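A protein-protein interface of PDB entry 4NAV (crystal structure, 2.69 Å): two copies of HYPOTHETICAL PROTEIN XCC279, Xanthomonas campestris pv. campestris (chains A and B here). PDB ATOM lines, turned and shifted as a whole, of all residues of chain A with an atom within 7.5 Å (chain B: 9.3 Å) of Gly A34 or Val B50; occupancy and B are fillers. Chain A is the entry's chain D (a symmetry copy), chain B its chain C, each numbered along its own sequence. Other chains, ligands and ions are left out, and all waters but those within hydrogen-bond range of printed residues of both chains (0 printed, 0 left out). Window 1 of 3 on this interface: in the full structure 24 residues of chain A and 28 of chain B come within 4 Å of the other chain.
Positions printed for both chains: 31, 47 and 155. Of the 17 pairs that touch across the chains among the printed residues, none has its exchanged pair printed and touching as well.
OD1 of Asn B49 is in hydrogen-bond range of N of Leu B51 (2.6 Å). N of Arg B160 lies within hydrogen-bond range of OD1 of Asp B52, at 2.8 Å. OE1 of Gln B58 lies within hydrogen-bond range of NE2 of Gln B54, at 3.2 Å. The side-chain carboxylate of Asp A26 sits close to the side-chain carboxylate of Asp A118, 2.6 Å away. The side-chain carboxylate (OD1) of Asp A118 lies close to the backbone carbonyl oxygen (O) of Asp A28 (2.7 Å). OD2 of Asp A33 lies within salt-bridge range of NE of Arg A35, 3.3 Å away.
O of Phe B48 is in hydrogen-bond range of N of Leu A36 (2.7 Å). N of Val B50 is in hydrogen-bond range of O of Gly A34. The guanidinium group (NH2) of Arg A35 is in salt-bridge range of the side-chain carboxylate (OE2) of Glu B156. The guanidinium group of Arg B160 is in salt-bridge range of the side-chain carboxylate of Asp A119.
Gly A34 touches just these residues of chain B: Phe B48, Asn B49 and Val B50. Printed residues of chain A within 4 Å of Val B50: Asp A28, Gly A34 and Leu A36. No residue of chain B comes within 4 Å of Asp A33. Of the printed residues of chain A, Gly B155 touches Arg A35 (3.7 Å). Printed residues of chain B within 4 Å of Asp A28: Val B50 (3.7 Å). Of the printed residues of chain A, Asn B49 touches Gly A34 (3.2 Å). Val A27 touches none of the printed residues of chain B. The nearest residue of chain B that does not touch Gly A34 is Leu B51 (5.1 Å).
Hydrophobic or aromatic side chains of chain A that line the printed part of chain B: Leu A36 and Tyr A37. Of the 20 printed residues of chain B, 10 touch a printed residue of chain A. Printed residues of chain B that touch a printed residue of chain A: Ala B47, Phe B48, Asn B49, Val B50, Leu B51, Gln B54, Arg B80, Gly B155, Glu B156 and Arg B160. Among the printed residues, 17 pairs touch across the chains.
Asp A28 touches Val B50 (CB to CG1, 3.7 Å). Phe B48 touches Gly A34. Asn B49 touches Gly A34 (CA to O, 3.2 Å). Ala B47 touches Arg A35 (CB to CD, 3.7 Å). Arg A35 touches Phe B48. Gly B155 touches Arg A35 (O to NH1, 3.7 Å). CD1 of Leu A36 touches CG1 of Val B50 (3.9 Å). Leu A36 touches Arg B80 (CD1 to NH1, 3.7 Å). Ala B47 touches Tyr A37 (CB to CE1, 3.7 Å). Leu B51 touches Asp A118.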
ATOM      1  N   ASP A  26     -13.747  10.915 -21.685  1.00  0.00           N
ATOM      2  CA  ASP A  26     -12.387  11.436 -21.702  1.00  0.00           C
ATOM      3  C   ASP A  26     -12.434  12.834 -22.308  1.00  0.00           C
ATOM      4  O   ASP A  26     -13.368  13.184 -23.015  1.00  0.00           O
ATOM      5  CB  ASP A  26     -11.494  10.551 -22.582  1.00  0.00           C
ATOM      6  CG  ASP A  26     -10.018  10.893 -22.460  1.00  0.00           C
ATOM      7  OD1 ASP A  26      -9.591  11.159 -21.303  1.00  0.00           O
ATOM      8  OD2 ASP A  26      -9.297  10.884 -23.499  1.00  0.00           O
ATOM      9  N   VAL A  27     -11.439  13.651 -22.039  1.00  0.00           N
ATOM     10  CA  VAL A  27     -11.390  14.981 -22.638  1.00  0.00           C
ATOM     11  C   VAL A  27     -10.577  14.924 -23.941  1.00  0.00           C
ATOM     12  O   VAL A  27     -11.126  15.044 -25.046  1.00  0.00           O
ATOM     13  CB  VAL A  27     -10.823  16.010 -21.634  1.00  0.00           C
ATOM     14  CG1 VAL A  27     -10.706  17.379 -22.267  1.00  0.00           C
ATOM     15  CG2 VAL A  27     -11.730  16.096 -20.409  1.00  0.00           C
ATOM     16  N   ASP A  28      -9.269  14.786 -23.790  1.00  0.00           N
ATOM     17  CA  ASP A  28      -8.376  14.884 -24.917  1.00  0.00           C
ATOM     18  C   ASP A  28      -8.431  13.688 -25.793  1.00  0.00           C
ATOM     19  O   ASP A  28      -8.271  12.540 -25.337  1.00  0.00           O
ATOM     20  CB  ASP A  28      -6.969  15.129 -24.444  1.00  0.00           C
ATOM     21  CG  ASP A  28      -6.770  16.557 -24.010  1.00  0.00           C
ATOM     22  OD1 ASP A  28      -6.774  17.469 -24.906  1.00  0.00           O
ATOM     23  OD2 ASP A  28      -6.580  16.749 -22.796  1.00  0.00           O
ATOM     24  N   GLY A  29      -8.668  13.986 -27.064  1.00  0.00           N
ATOM     25  CA  GLY A  29      -8.815  12.983 -28.096  1.00  0.00           C
ATOM     26  C   GLY A  29     -10.233  12.473 -28.267  1.00  0.00           C
ATOM     27  O   GLY A  29     -10.501  11.695 -29.188  1.00  0.00           O
ATOM     28  N   THR A  30     -11.136  12.910 -27.394  1.00  0.00           N
ATOM     29  CA  THR A  30     -12.493  12.397 -27.344  1.00  0.00           C
ATOM     30  C   THR A  30     -13.494  13.530 -27.549  1.00  0.00           C
ATOM     31  O   THR A  30     -14.289  13.489 -28.497  1.00  0.00           O
ATOM     32  CB  THR A  30     -12.703  11.718 -25.999  1.00  0.00           C
ATOM     33  OG1 THR A  30     -11.979  10.490 -25.990  1.00  0.00           O
ATOM     34  CG2 THR A  30     -14.145  11.438 -25.750  1.00  0.00           C
ATOM     35  N   LEU A  31     -13.401  14.564 -26.708  1.00  0.00           N
ATOM     36  CA  LEU A  31     -14.065  15.864 -26.972  1.00  0.00           C
ATOM     37  C   LEU A  31     -13.165  16.860 -27.711  1.00  0.00           C
ATOM     38  O   LEU A  31     -13.534  18.009 -27.936  1.00  0.00           O
ATOM     39  CB  LEU A  31     -14.481  16.500 -25.655  1.00  0.00           C
ATOM     40  CG  LEU A  31     -15.306  15.606 -24.755  1.00  0.00           C
ATOM     41  CD1 LEU A  31     -15.487  16.267 -23.401  1.00  0.00           C
ATOM     42  CD2 LEU A  31     -16.643  15.313 -25.392  1.00  0.00           C
ATOM     43  N   THR A  32     -11.968  16.408 -28.057  1.00  0.00           N
ATOM     44  CA  THR A  32     -10.892  17.254 -28.584  1.00  0.00           C
ATOM     45  C   THR A  32     -10.274  16.408 -29.659  1.00  0.00           C
ATOM     46  O   THR A  32     -10.401  15.191 -29.631  1.00  0.00           O
ATOM     47  CB  THR A  32      -9.925  17.565 -27.428  1.00  0.00           C
ATOM     48  OG1 THR A  32     -10.453  18.663 -26.664  1.00  0.00           O
ATOM     49  CG2 THR A  32      -8.537  17.892 -27.852  1.00  0.00           C
ATOM     50  N   ASP A  33      -9.619  17.041 -30.619  1.00  0.00           N
ATOM     51  CA  ASP A  33      -8.891  16.314 -31.686  1.00  0.00           C
ATOM     52  C   ASP A  33      -7.486  15.855 -31.260  1.00  0.00           C
ATOM     53  O   ASP A  33      -6.642  15.530 -32.110  1.00  0.00           O
ATOM     54  CB  ASP A  33      -8.788  17.177 -32.948  1.00  0.00           C
ATOM     55  CG  ASP A  33      -8.135  18.530 -32.692  1.00  0.00           C
ATOM     56  OD1 ASP A  33      -7.667  18.788 -31.569  1.00  0.00           O
ATOM     57  OD2 ASP A  33      -8.140  19.353 -33.624  1.00  0.00           O
ATOM     58  N   GLY A  34      -7.244  15.888 -29.949  1.00  0.00           N
ATOM     59  CA  GLY A  34      -6.000  15.518 -29.350  1.00  0.00           C
ATOM     60  C   GLY A  34      -4.994  16.663 -29.225  1.00  0.00           C
ATOM     61  O   GLY A  34      -3.890  16.475 -28.691  1.00  0.00           O
ATOM     62  N   ARG A  35      -5.331  17.830 -29.743  1.00  0.00           N
ATOM     63  CA  ARG A  35      -4.381  18.938 -29.773  1.00  0.00           C
ATOM     64  C   ARG A  35      -4.322  19.734 -28.468  1.00  0.00           C
ATOM     65  O   ARG A  35      -5.344  20.007 -27.867  1.00  0.00           O
ATOM     66  CB  ARG A  35      -4.714  19.886 -30.929  1.00  0.00           C
ATOM     67  CG  ARG A  35      -3.926  19.630 -32.185  1.00  0.00           C
ATOM     68  CD  ARG A  35      -4.409  20.543 -33.284  1.00  0.00           C
ATOM     69  NE  ARG A  35      -4.987  19.736 -34.356  1.00  0.00           N
ATOM     70  CZ  ARG A  35      -4.380  19.253 -35.441  1.00  0.00           C
ATOM     71  NH1 ARG A  35      -3.089  19.474 -35.729  1.00  0.00           N
ATOM     72  NH2 ARG A  35      -5.123  18.519 -36.265  1.00  0.00           N
ATOM     73  N   LEU A  36      -3.110  20.077 -28.047  1.00  0.00           N
ATOM     74  CA  LEU A  36      -2.845  21.034 -26.970  1.00  0.00           C
ATOM     75  C   LEU A  36      -2.077  22.243 -27.507  1.00  0.00           C
ATOM     76  O   LEU A  36      -0.942  22.125 -27.973  1.00  0.00           O
ATOM     77  CB  LEU A  36      -2.012  20.398 -25.875  1.00  0.00           C
ATOM     78  CG  LEU A  36      -2.742  19.396 -24.990  1.00  0.00           C
ATOM     79  CD1 LEU A  36      -1.777  18.733 -24.014  1.00  0.00           C
ATOM     80  CD2 LEU A  36      -3.858  20.090 -24.220  1.00  0.00           C
ATOM     81  N   TYR A  37      -2.720  23.401 -27.433  1.00  0.00           N
ATOM     82  CA  TYR A  37      -2.134  24.628 -27.903  1.00  0.00           C
ATOM     83  C   TYR A  37      -1.322  25.230 -26.737  1.00  0.00           C
ATOM     84  O   TYR A  37      -1.874  25.574 -25.679  1.00  0.00           O
ATOM     85  CB  TYR A  37      -3.226  25.590 -28.378  1.00  0.00           C
ATOM     86  CG  TYR A  37      -4.025  25.023 -29.510  1.00  0.00           C
ATOM     87  CD1 TYR A  37      -3.753  25.375 -30.804  1.00  0.00           C
ATOM     88  CD2 TYR A  37      -5.068  24.110 -29.280  1.00  0.00           C
ATOM     89  CE1 TYR A  37      -4.469  24.853 -31.851  1.00  0.00           C
ATOM     90  CE2 TYR A  37      -5.789  23.588 -30.320  1.00  0.00           C
ATOM     91  CZ  TYR A  37      -5.488  23.960 -31.610  1.00  0.00           C
ATOM     92  OH  TYR A  37      -6.163  23.435 -32.689  1.00  0.00           O
ATOM     93  N   GLU A  44      -1.824  26.399 -21.570  1.00  0.00           N
ATOM     94  CA  GLU A  44      -2.456  25.468 -22.511  1.00  0.00           C
ATOM     95  C   GLU A  44      -3.922  25.793 -22.861  1.00  0.00           C
ATOM     96  O   GLU A  44      -4.660  26.299 -22.025  1.00  0.00           O
ATOM     97  CB  GLU A  44      -2.379  24.044 -21.952  1.00  0.00           C
ATOM     98  CG  GLU A  44      -0.949  23.555 -21.759  1.00  0.00           C
ATOM     99  CD  GLU A  44      -0.889  22.179 -21.132  1.00  0.00           C
ATOM    100  OE1 GLU A  44      -1.885  21.438 -21.227  1.00  0.00           O
ATOM    101  OE2 GLU A  44       0.151  21.830 -20.546  1.00  0.00           O
ATOM    102  N   LYS A  46      -7.356  24.016 -25.368  1.00  0.00           N
ATOM    103  CA  LYS A  46      -7.884  22.874 -26.124  1.00  0.00           C
ATOM    104  C   LYS A  46      -9.068  23.367 -26.912  1.00  0.00           C
ATOM    105  O   LYS A  46      -9.643  24.376 -26.562  1.00  0.00           O
ATOM    106  CB  LYS A  46      -8.349  21.739 -25.204  1.00  0.00           C
ATOM    107  CG  LYS A  46      -7.641  21.667 -23.853  1.00  0.00           C
ATOM    108  CD  LYS A  46      -7.998  20.418 -23.061  1.00  0.00           C
ATOM    109  CE  LYS A  46      -6.838  19.998 -22.171  1.00  0.00           C
ATOM    110  NZ  LYS A  46      -7.262  19.147 -21.014  1.00  0.00           N
ATOM    111  N   ALA A  47      -9.443  22.645 -27.964  1.00  0.00           N
ATOM    112  CA  ALA A  47     -10.630  22.984 -28.713  1.00  0.00           C
ATOM    113  C   ALA A  47     -11.728  21.966 -28.498  1.00  0.00           C
ATOM    114  O   ALA A  47     -11.592  20.789 -28.862  1.00  0.00           O
ATOM    115  CB  ALA A  47     -10.315  23.089 -30.180  1.00  0.00           C
ATOM    116  N   ASP A 118     -10.070   7.482 -25.838  1.00  0.00           N
ATOM    117  CA  ASP A 118      -9.274   7.317 -27.064  1.00  0.00           C
ATOM    118  C   ASP A 118      -7.901   6.664 -26.884  1.00  0.00           C
ATOM    119  O   ASP A 118      -7.298   6.271 -27.878  1.00  0.00           O
ATOM    120  CB  ASP A 118      -9.070   8.681 -27.723  1.00  0.00           C
ATOM    121  CG  ASP A 118      -8.183   9.599 -26.910  1.00  0.00           C
ATOM    122  OD1 ASP A 118      -8.465   9.833 -25.706  1.00  0.00           O
ATOM    123  OD2 ASP A 118      -7.180  10.087 -27.494  1.00  0.00           O
ATOM    124  N   ASP A 119      -7.409   6.549 -25.647  1.00  0.00           N
ATOM    125  CA  ASP A 119      -6.023   6.083 -25.388  1.00  0.00           C
ATOM    126  C   ASP A 119      -5.875   5.311 -24.070  1.00  0.00           C
ATOM    127  O   ASP A 119      -6.818   5.194 -23.296  1.00  0.00           O
ATOM    128  CB  ASP A 119      -5.047   7.285 -25.431  1.00  0.00           C
ATOM    129  CG  ASP A 119      -3.629   6.909 -25.852  1.00  0.00           C
ATOM    130  OD1 ASP A 119      -3.366   5.718 -26.167  1.00  0.00           O
ATOM    131  OD2 ASP A 119      -2.751   7.820 -25.867  1.00  0.00           O
ATOM    132  N   ASN A 137     -10.586   8.416 -34.483  1.00  0.00           N
ATOM    133  CA  ASN A 137      -9.149   8.688 -34.304  1.00  0.00           C
ATOM    134  C   ASN A 137      -8.485   7.931 -33.156  1.00  0.00           C
ATOM    135  O   ASN A 137      -7.357   8.221 -32.811  1.00  0.00           O
ATOM    136  CB  ASN A 137      -8.932  10.201 -34.062  1.00  0.00           C
ATOM    137  CG  ASN A 137      -9.749  10.708 -32.896  1.00  0.00           C
ATOM    138  OD1 ASN A 137     -10.980  10.733 -32.990  1.00  0.00           O
ATOM    139  ND2 ASN A 137      -9.093  11.090 -31.779  1.00  0.00           N
ATOM    140  N   GLY A 154     -12.698  12.594 -32.826  1.00  0.00           N
ATOM    141  CA  GLY A 154     -12.738  13.356 -31.594  1.00  0.00           C
ATOM    142  C   GLY A 154     -12.591  14.806 -31.935  1.00  0.00           C
ATOM    143  O   GLY A 154     -11.785  15.172 -32.781  1.00  0.00           O
ATOM    144  N   GLY A 155     -13.426  15.625 -31.334  1.00  0.00           N
ATOM    145  CA  GLY A 155     -13.379  17.069 -31.559  1.00  0.00           C
ATOM    146  C   GLY A 155     -14.002  17.494 -32.882  1.00  0.00           C
ATOM    147  O   GLY A 155     -13.940  18.675 -33.247  1.00  0.00           O
ATOM    148  N   LEU B  31       6.142  17.149 -34.101  1.00  0.00           N
ATOM    149  CA  LEU B  31       5.169  17.099 -32.988  1.00  0.00           C
ATOM    150  C   LEU B  31       4.031  18.088 -33.171  1.00  0.00           C
ATOM    151  O   LEU B  31       3.156  18.210 -32.329  1.00  0.00           O
ATOM    152  CB  LEU B  31       5.856  17.424 -31.681  1.00  0.00           C
ATOM    153  CG  LEU B  31       7.099  16.600 -31.375  1.00  0.00           C
ATOM    154  CD1 LEU B  31       7.799  17.167 -30.151  1.00  0.00           C
ATOM    155  CD2 LEU B  31       6.739  15.144 -31.151  1.00  0.00           C
ATOM    156  N   ALA B  47       0.456  23.754 -31.550  1.00  0.00           N
ATOM    157  CA  ALA B  47      -0.334  22.669 -31.039  1.00  0.00           C
ATOM    158  C   ALA B  47       0.456  21.350 -30.994  1.00  0.00           C
ATOM    159  O   ALA B  47       0.818  20.809 -32.032  1.00  0.00           O
ATOM    160  CB  ALA B  47      -1.599  22.512 -31.886  1.00  0.00           C
ATOM    161  N   PHE B  48       0.616  20.794 -29.803  1.00  0.00           N
ATOM    162  CA  PHE B  48       1.069  19.405 -29.638  1.00  0.00           C
ATOM    163  C   PHE B  48      -0.116  18.470 -29.553  1.00  0.00           C
ATOM    164  O   PHE B  48      -1.238  18.932 -29.537  1.00  0.00           O
ATOM    165  CB  PHE B  48       1.948  19.304 -28.402  1.00  0.00           C
ATOM    166  CG  PHE B  48       3.130  20.209 -28.469  1.00  0.00           C
ATOM    167  CD1 PHE B  48       4.300  19.783 -29.058  1.00  0.00           C
ATOM    168  CD2 PHE B  48       3.049  21.505 -28.019  1.00  0.00           C
ATOM    169  CE1 PHE B  48       5.396  20.619 -29.134  1.00  0.00           C
ATOM    170  CE2 PHE B  48       4.129  22.357 -28.099  1.00  0.00           C
ATOM    171  CZ  PHE B  48       5.305  21.913 -28.655  1.00  0.00           C
ATOM    172  N   ASN B  49       0.156  17.165 -29.481  1.00  0.00           N
ATOM    173  CA  ASN B  49      -0.862  16.091 -29.533  1.00  0.00           C
ATOM    174  C   ASN B  49      -0.745  15.133 -28.348  1.00  0.00           C
ATOM    175  O   ASN B  49       0.358  14.697 -28.048  1.00  0.00           O
ATOM    176  CB  ASN B  49      -0.628  15.280 -30.792  1.00  0.00           C
ATOM    177  CG  ASN B  49      -1.577  14.102 -30.918  1.00  0.00           C
ATOM    178  OD1 ASN B  49      -1.411  13.079 -30.245  1.00  0.00           O
ATOM    179  ND2 ASN B  49      -2.575  14.240 -31.790  1.00  0.00           N
ATOM    180  N   VAL B  50      -1.855  14.791 -27.683  1.00  0.00           N
ATOM    181  CA  VAL B  50      -1.756  13.976 -26.476  1.00  0.00           C
ATOM    182  C   VAL B  50      -1.325  12.541 -26.734  1.00  0.00           C
ATOM    183  O   VAL B  50      -0.715  11.945 -25.858  1.00  0.00           O
ATOM    184  CB  VAL B  50      -3.036  13.929 -25.631  1.00  0.00           C
ATOM    185  CG1 VAL B  50      -3.373  15.325 -25.146  1.00  0.00           C
ATOM    186  CG2 VAL B  50      -4.193  13.274 -26.407  1.00  0.00           C
ATOM    187  N   LEU B  51      -1.653  11.977 -27.893  1.00  0.00           N
ATOM    188  CA  LEU B  51      -1.169  10.648 -28.214  1.00  0.00           C
ATOM    189  C   LEU B  51       0.348  10.677 -28.323  1.00  0.00           C
ATOM    190  O   LEU B  51       1.036   9.758 -27.866  1.00  0.00           O
ATOM    191  CB  LEU B  51      -1.758  10.116 -29.513  1.00  0.00           C
ATOM    192  CG  LEU B  51      -3.284   9.984 -29.596  1.00  0.00           C
ATOM    193  CD1 LEU B  51      -3.716   9.412 -30.955  1.00  0.00           C
ATOM    194  CD2 LEU B  51      -3.867   9.161 -28.459  1.00  0.00           C
ATOM    195  N   ASP B  52       0.865  11.716 -28.954  1.00  0.00           N
ATOM    196  CA  ASP B  52       2.308  11.904 -29.007  1.00  0.00           C
ATOM    197  C   ASP B  52       2.895  11.973 -27.584  1.00  0.00           C
ATOM    198  O   ASP B  52       3.849  11.277 -27.266  1.00  0.00           O
ATOM    199  CB  ASP B  52       2.686  13.140 -29.869  1.00  0.00           C
ATOM    200  CG  ASP B  52       2.405  12.923 -31.393  1.00  0.00           C
ATOM    201  OD1 ASP B  52       2.283  11.757 -31.850  1.00  0.00           O
ATOM    202  OD2 ASP B  52       2.281  13.919 -32.130  1.00  0.00           O
ATOM    203  N   GLY B  53       2.254  12.745 -26.705  1.00  0.00           N
ATOM    204  CA  GLY B  53       2.662  12.840 -25.302  1.00  0.00           C
ATOM    205  C   GLY B  53       2.694  11.506 -24.577  1.00  0.00           C
ATOM    206  O   GLY B  53       3.675  11.172 -23.901  1.00  0.00           O
ATOM    207  N   GLN B  54       1.634  10.735 -24.713  1.00  0.00           N
ATOM    208  CA  GLN B  54       1.594   9.414 -24.115  1.00  0.00           C
ATOM    209  C   GLN B  54       2.728   8.566 -24.663  1.00  0.00           C
ATOM    210  O   GLN B  54       3.401   7.888 -23.914  1.00  0.00           O
ATOM    211  CB  GLN B  54       0.226   8.748 -24.361  1.00  0.00           C
ATOM    212  CG  GLN B  54      -0.020   7.442 -23.609  1.00  0.00           C
ATOM    213  CD  GLN B  54       0.144   7.591 -22.096  1.00  0.00           C
ATOM    214  OE1 GLN B  54      -0.534   8.391 -21.463  1.00  0.00           O
ATOM    215  NE2 GLN B  54       1.047   6.811 -21.520  1.00  0.00           N
ATOM    216  N   GLY B  55       2.981   8.632 -25.960  1.00  0.00           N
ATOM    217  CA  GLY B  55       4.090   7.863 -26.529  1.00  0.00           C
ATOM    218  C   GLY B  55       5.451   8.232 -25.967  1.00  0.00           C
ATOM    219  O   GLY B  55       6.284   7.379 -25.691  1.00  0.00           O
ATOM    220  N   LEU B  56       5.680   9.518 -25.781  1.00  0.00           N
ATOM    221  CA  LEU B  56       6.982   9.972 -25.364  1.00  0.00           C
ATOM    222  C   LEU B  56       7.322   9.565 -23.919  1.00  0.00           C
ATOM    223  O   LEU B  56       8.440   9.149 -23.634  1.00  0.00           O
ATOM    224  CB  LEU B  56       7.076  11.481 -25.570  1.00  0.00           C
ATOM    225  CG  LEU B  56       7.041  11.888 -27.059  1.00  0.00           C
ATOM    226  CD1 LEU B  56       6.868  13.398 -27.196  1.00  0.00           C
ATOM    227  CD2 LEU B  56       8.280  11.431 -27.817  1.00  0.00           C
ATOM    228  N   LYS B  57       6.346   9.701 -23.029  1.00  0.00           N
ATOM    229  CA  LYS B  57       6.451   9.222 -21.659  1.00  0.00           C
ATOM    230  C   LYS B  57       6.795   7.737 -21.622  1.00  0.00           C
ATOM    231  O   LYS B  57       7.615   7.294 -20.818  1.00  0.00           O
ATOM    232  CB  LYS B  57       5.120   9.457 -20.924  1.00  0.00           C
ATOM    233  CG  LYS B  57       4.952  10.906 -20.447  1.00  0.00           C
ATOM    234  CD  LYS B  57       3.678  11.383 -19.719  1.00  0.00           C
ATOM    235  CE  LYS B  57       2.323  11.084 -20.375  1.00  0.00           C
ATOM    236  NZ  LYS B  57       1.136  11.393 -19.515  1.00  0.00           N
ATOM    237  N   GLN B  58       6.212   6.971 -22.531  1.00  0.00           N
ATOM    238  CA  GLN B  58       6.400   5.522 -22.536  1.00  0.00           C
ATOM    239  C   GLN B  58       7.800   5.132 -22.950  1.00  0.00           C
ATOM    240  O   GLN B  58       8.376   4.193 -22.400  1.00  0.00           O
ATOM    241  CB  GLN B  58       5.405   4.881 -23.462  1.00  0.00           C
ATOM    242  CG  GLN B  58       3.987   5.175 -22.995  1.00  0.00           C
ATOM    243  CD  GLN B  58       3.549   4.270 -21.863  1.00  0.00           C
ATOM    244  OE1 GLN B  58       3.283   4.705 -20.728  1.00  0.00           O
ATOM    245  NE2 GLN B  58       3.444   3.001 -22.178  1.00  0.00           N
ATOM    246  N   ARG B  80       6.689  22.258 -22.795  1.00  0.00           N
ATOM    247  CA  ARG B  80       6.211  20.954 -23.247  1.00  0.00           C
ATOM    248  C   ARG B  80       7.099  19.811 -22.778  1.00  0.00           C
ATOM    249  O   ARG B  80       6.616  18.778 -22.332  1.00  0.00           O
ATOM    250  CB  ARG B  80       6.105  20.945 -24.782  1.00  0.00           C
ATOM    251  CG  ARG B  80       5.524  19.669 -25.386  1.00  0.00           C
ATOM    252  CD  ARG B  80       4.160  19.320 -24.822  1.00  0.00           C
ATOM    253  NE  ARG B  80       3.650  18.083 -25.405  1.00  0.00           N
ATOM    254  CZ  ARG B  80       2.550  17.447 -25.007  1.00  0.00           C
ATOM    255  NH1 ARG B  80       1.804  17.924 -24.012  1.00  0.00           N
ATOM    256  NH2 ARG B  80       2.184  16.331 -25.624  1.00  0.00           N
ATOM    257  N   LEU B  84       6.239  16.584 -19.891  1.00  0.00           N
ATOM    258  CA  LEU B  84       6.386  15.157 -20.188  1.00  0.00           C
ATOM    259  C   LEU B  84       7.639  14.543 -19.577  1.00  0.00           C
ATOM    260  O   LEU B  84       7.811  13.320 -19.636  1.00  0.00           O
ATOM    261  CB  LEU B  84       6.402  14.927 -21.709  1.00  0.00           C
ATOM    262  CG  LEU B  84       5.189  15.446 -22.491  1.00  0.00           C
ATOM    263  CD1 LEU B  84       5.453  15.418 -23.978  1.00  0.00           C
ATOM    264  CD2 LEU B  84       3.937  14.656 -22.150  1.00  0.00           C
ATOM    265  N   GLY B 155       1.782  16.090 -35.655  1.00  0.00           N
ATOM    266  CA  GLY B 155       0.768  16.749 -34.819  1.00  0.00           C
ATOM    267  C   GLY B 155      -0.554  16.007 -34.836  1.00  0.00           C
ATOM    268  O   GLY B 155      -1.531  16.483 -34.267  1.00  0.00           O
ATOM    269  N   GLU B 156      -0.571  14.845 -35.507  1.00  0.00           N
ATOM    270  CA  GLU B 156      -1.740  13.963 -35.571  1.00  0.00           C
ATOM    271  C   GLU B 156      -1.325  12.510 -35.280  1.00  0.00           C
ATOM    272  O   GLU B 156      -1.841  11.572 -35.862  1.00  0.00           O
ATOM    273  CB  GLU B 156      -2.402  14.091 -36.934  1.00  0.00           C
ATOM    274  CG  GLU B 156      -2.994  15.475 -37.180  1.00  0.00           C
ATOM    275  CD  GLU B 156      -3.540  15.691 -38.608  1.00  0.00           C
ATOM    276  OE1 GLU B 156      -3.601  14.728 -39.420  1.00  0.00           O
ATOM    277  OE2 GLU B 156      -3.885  16.849 -38.933  1.00  0.00           O
ATOM    278  N   GLY B 157      -0.364  12.336 -34.375  1.00  0.00           N
ATOM    279  CA  GLY B 157       0.053  11.010 -33.918  1.00  0.00           C
ATOM    280  C   GLY B 157       1.283  10.405 -34.568  1.00  0.00           C
ATOM    281  O   GLY B 157       1.594   9.248 -34.325  1.00  0.00           O
ATOM    282  N   ALA B 159       4.435  11.017 -34.084  1.00  0.00           N
ATOM    283  CA  ALA B 159       5.436  10.672 -33.098  1.00  0.00           C
ATOM    284  C   ALA B 159       5.012   9.454 -32.255  1.00  0.00           C
ATOM    285  O   ALA B 159       5.839   8.610 -31.901  1.00  0.00           O
ATOM    286  CB  ALA B 159       5.722  11.863 -32.226  1.00  0.00           C
ATOM    287  N   ARG B 160       3.728   9.344 -31.926  1.00  0.00           N
ATOM    288  CA  ARG B 160       3.258   8.165 -31.233  1.00  0.00           C
ATOM    289  C   ARG B 160       3.525   6.963 -32.095  1.00  0.00           C
ATOM    290  O   ARG B 160       3.970   5.922 -31.613  1.00  0.00           O
ATOM    291  CB  ARG B 160       1.755   8.263 -30.939  1.00  0.00           C
ATOM    292  CG  ARG B 160       1.150   7.015 -30.315  1.00  0.00           C
ATOM    293  CD  ARG B 160       1.900   6.585 -29.070  1.00  0.00           C
ATOM    294  NE  ARG B 160       1.179   5.569 -28.317  1.00  0.00           N
ATOM    295  CZ  ARG B 160       0.105   5.798 -27.566  1.00  0.00           C
ATOM    296  NH1 ARG B 160      -0.400   7.025 -27.434  1.00  0.00           N
ATOM    297  NH2 ARG B 160      -0.488   4.792 -26.959  1.00  0.00           N
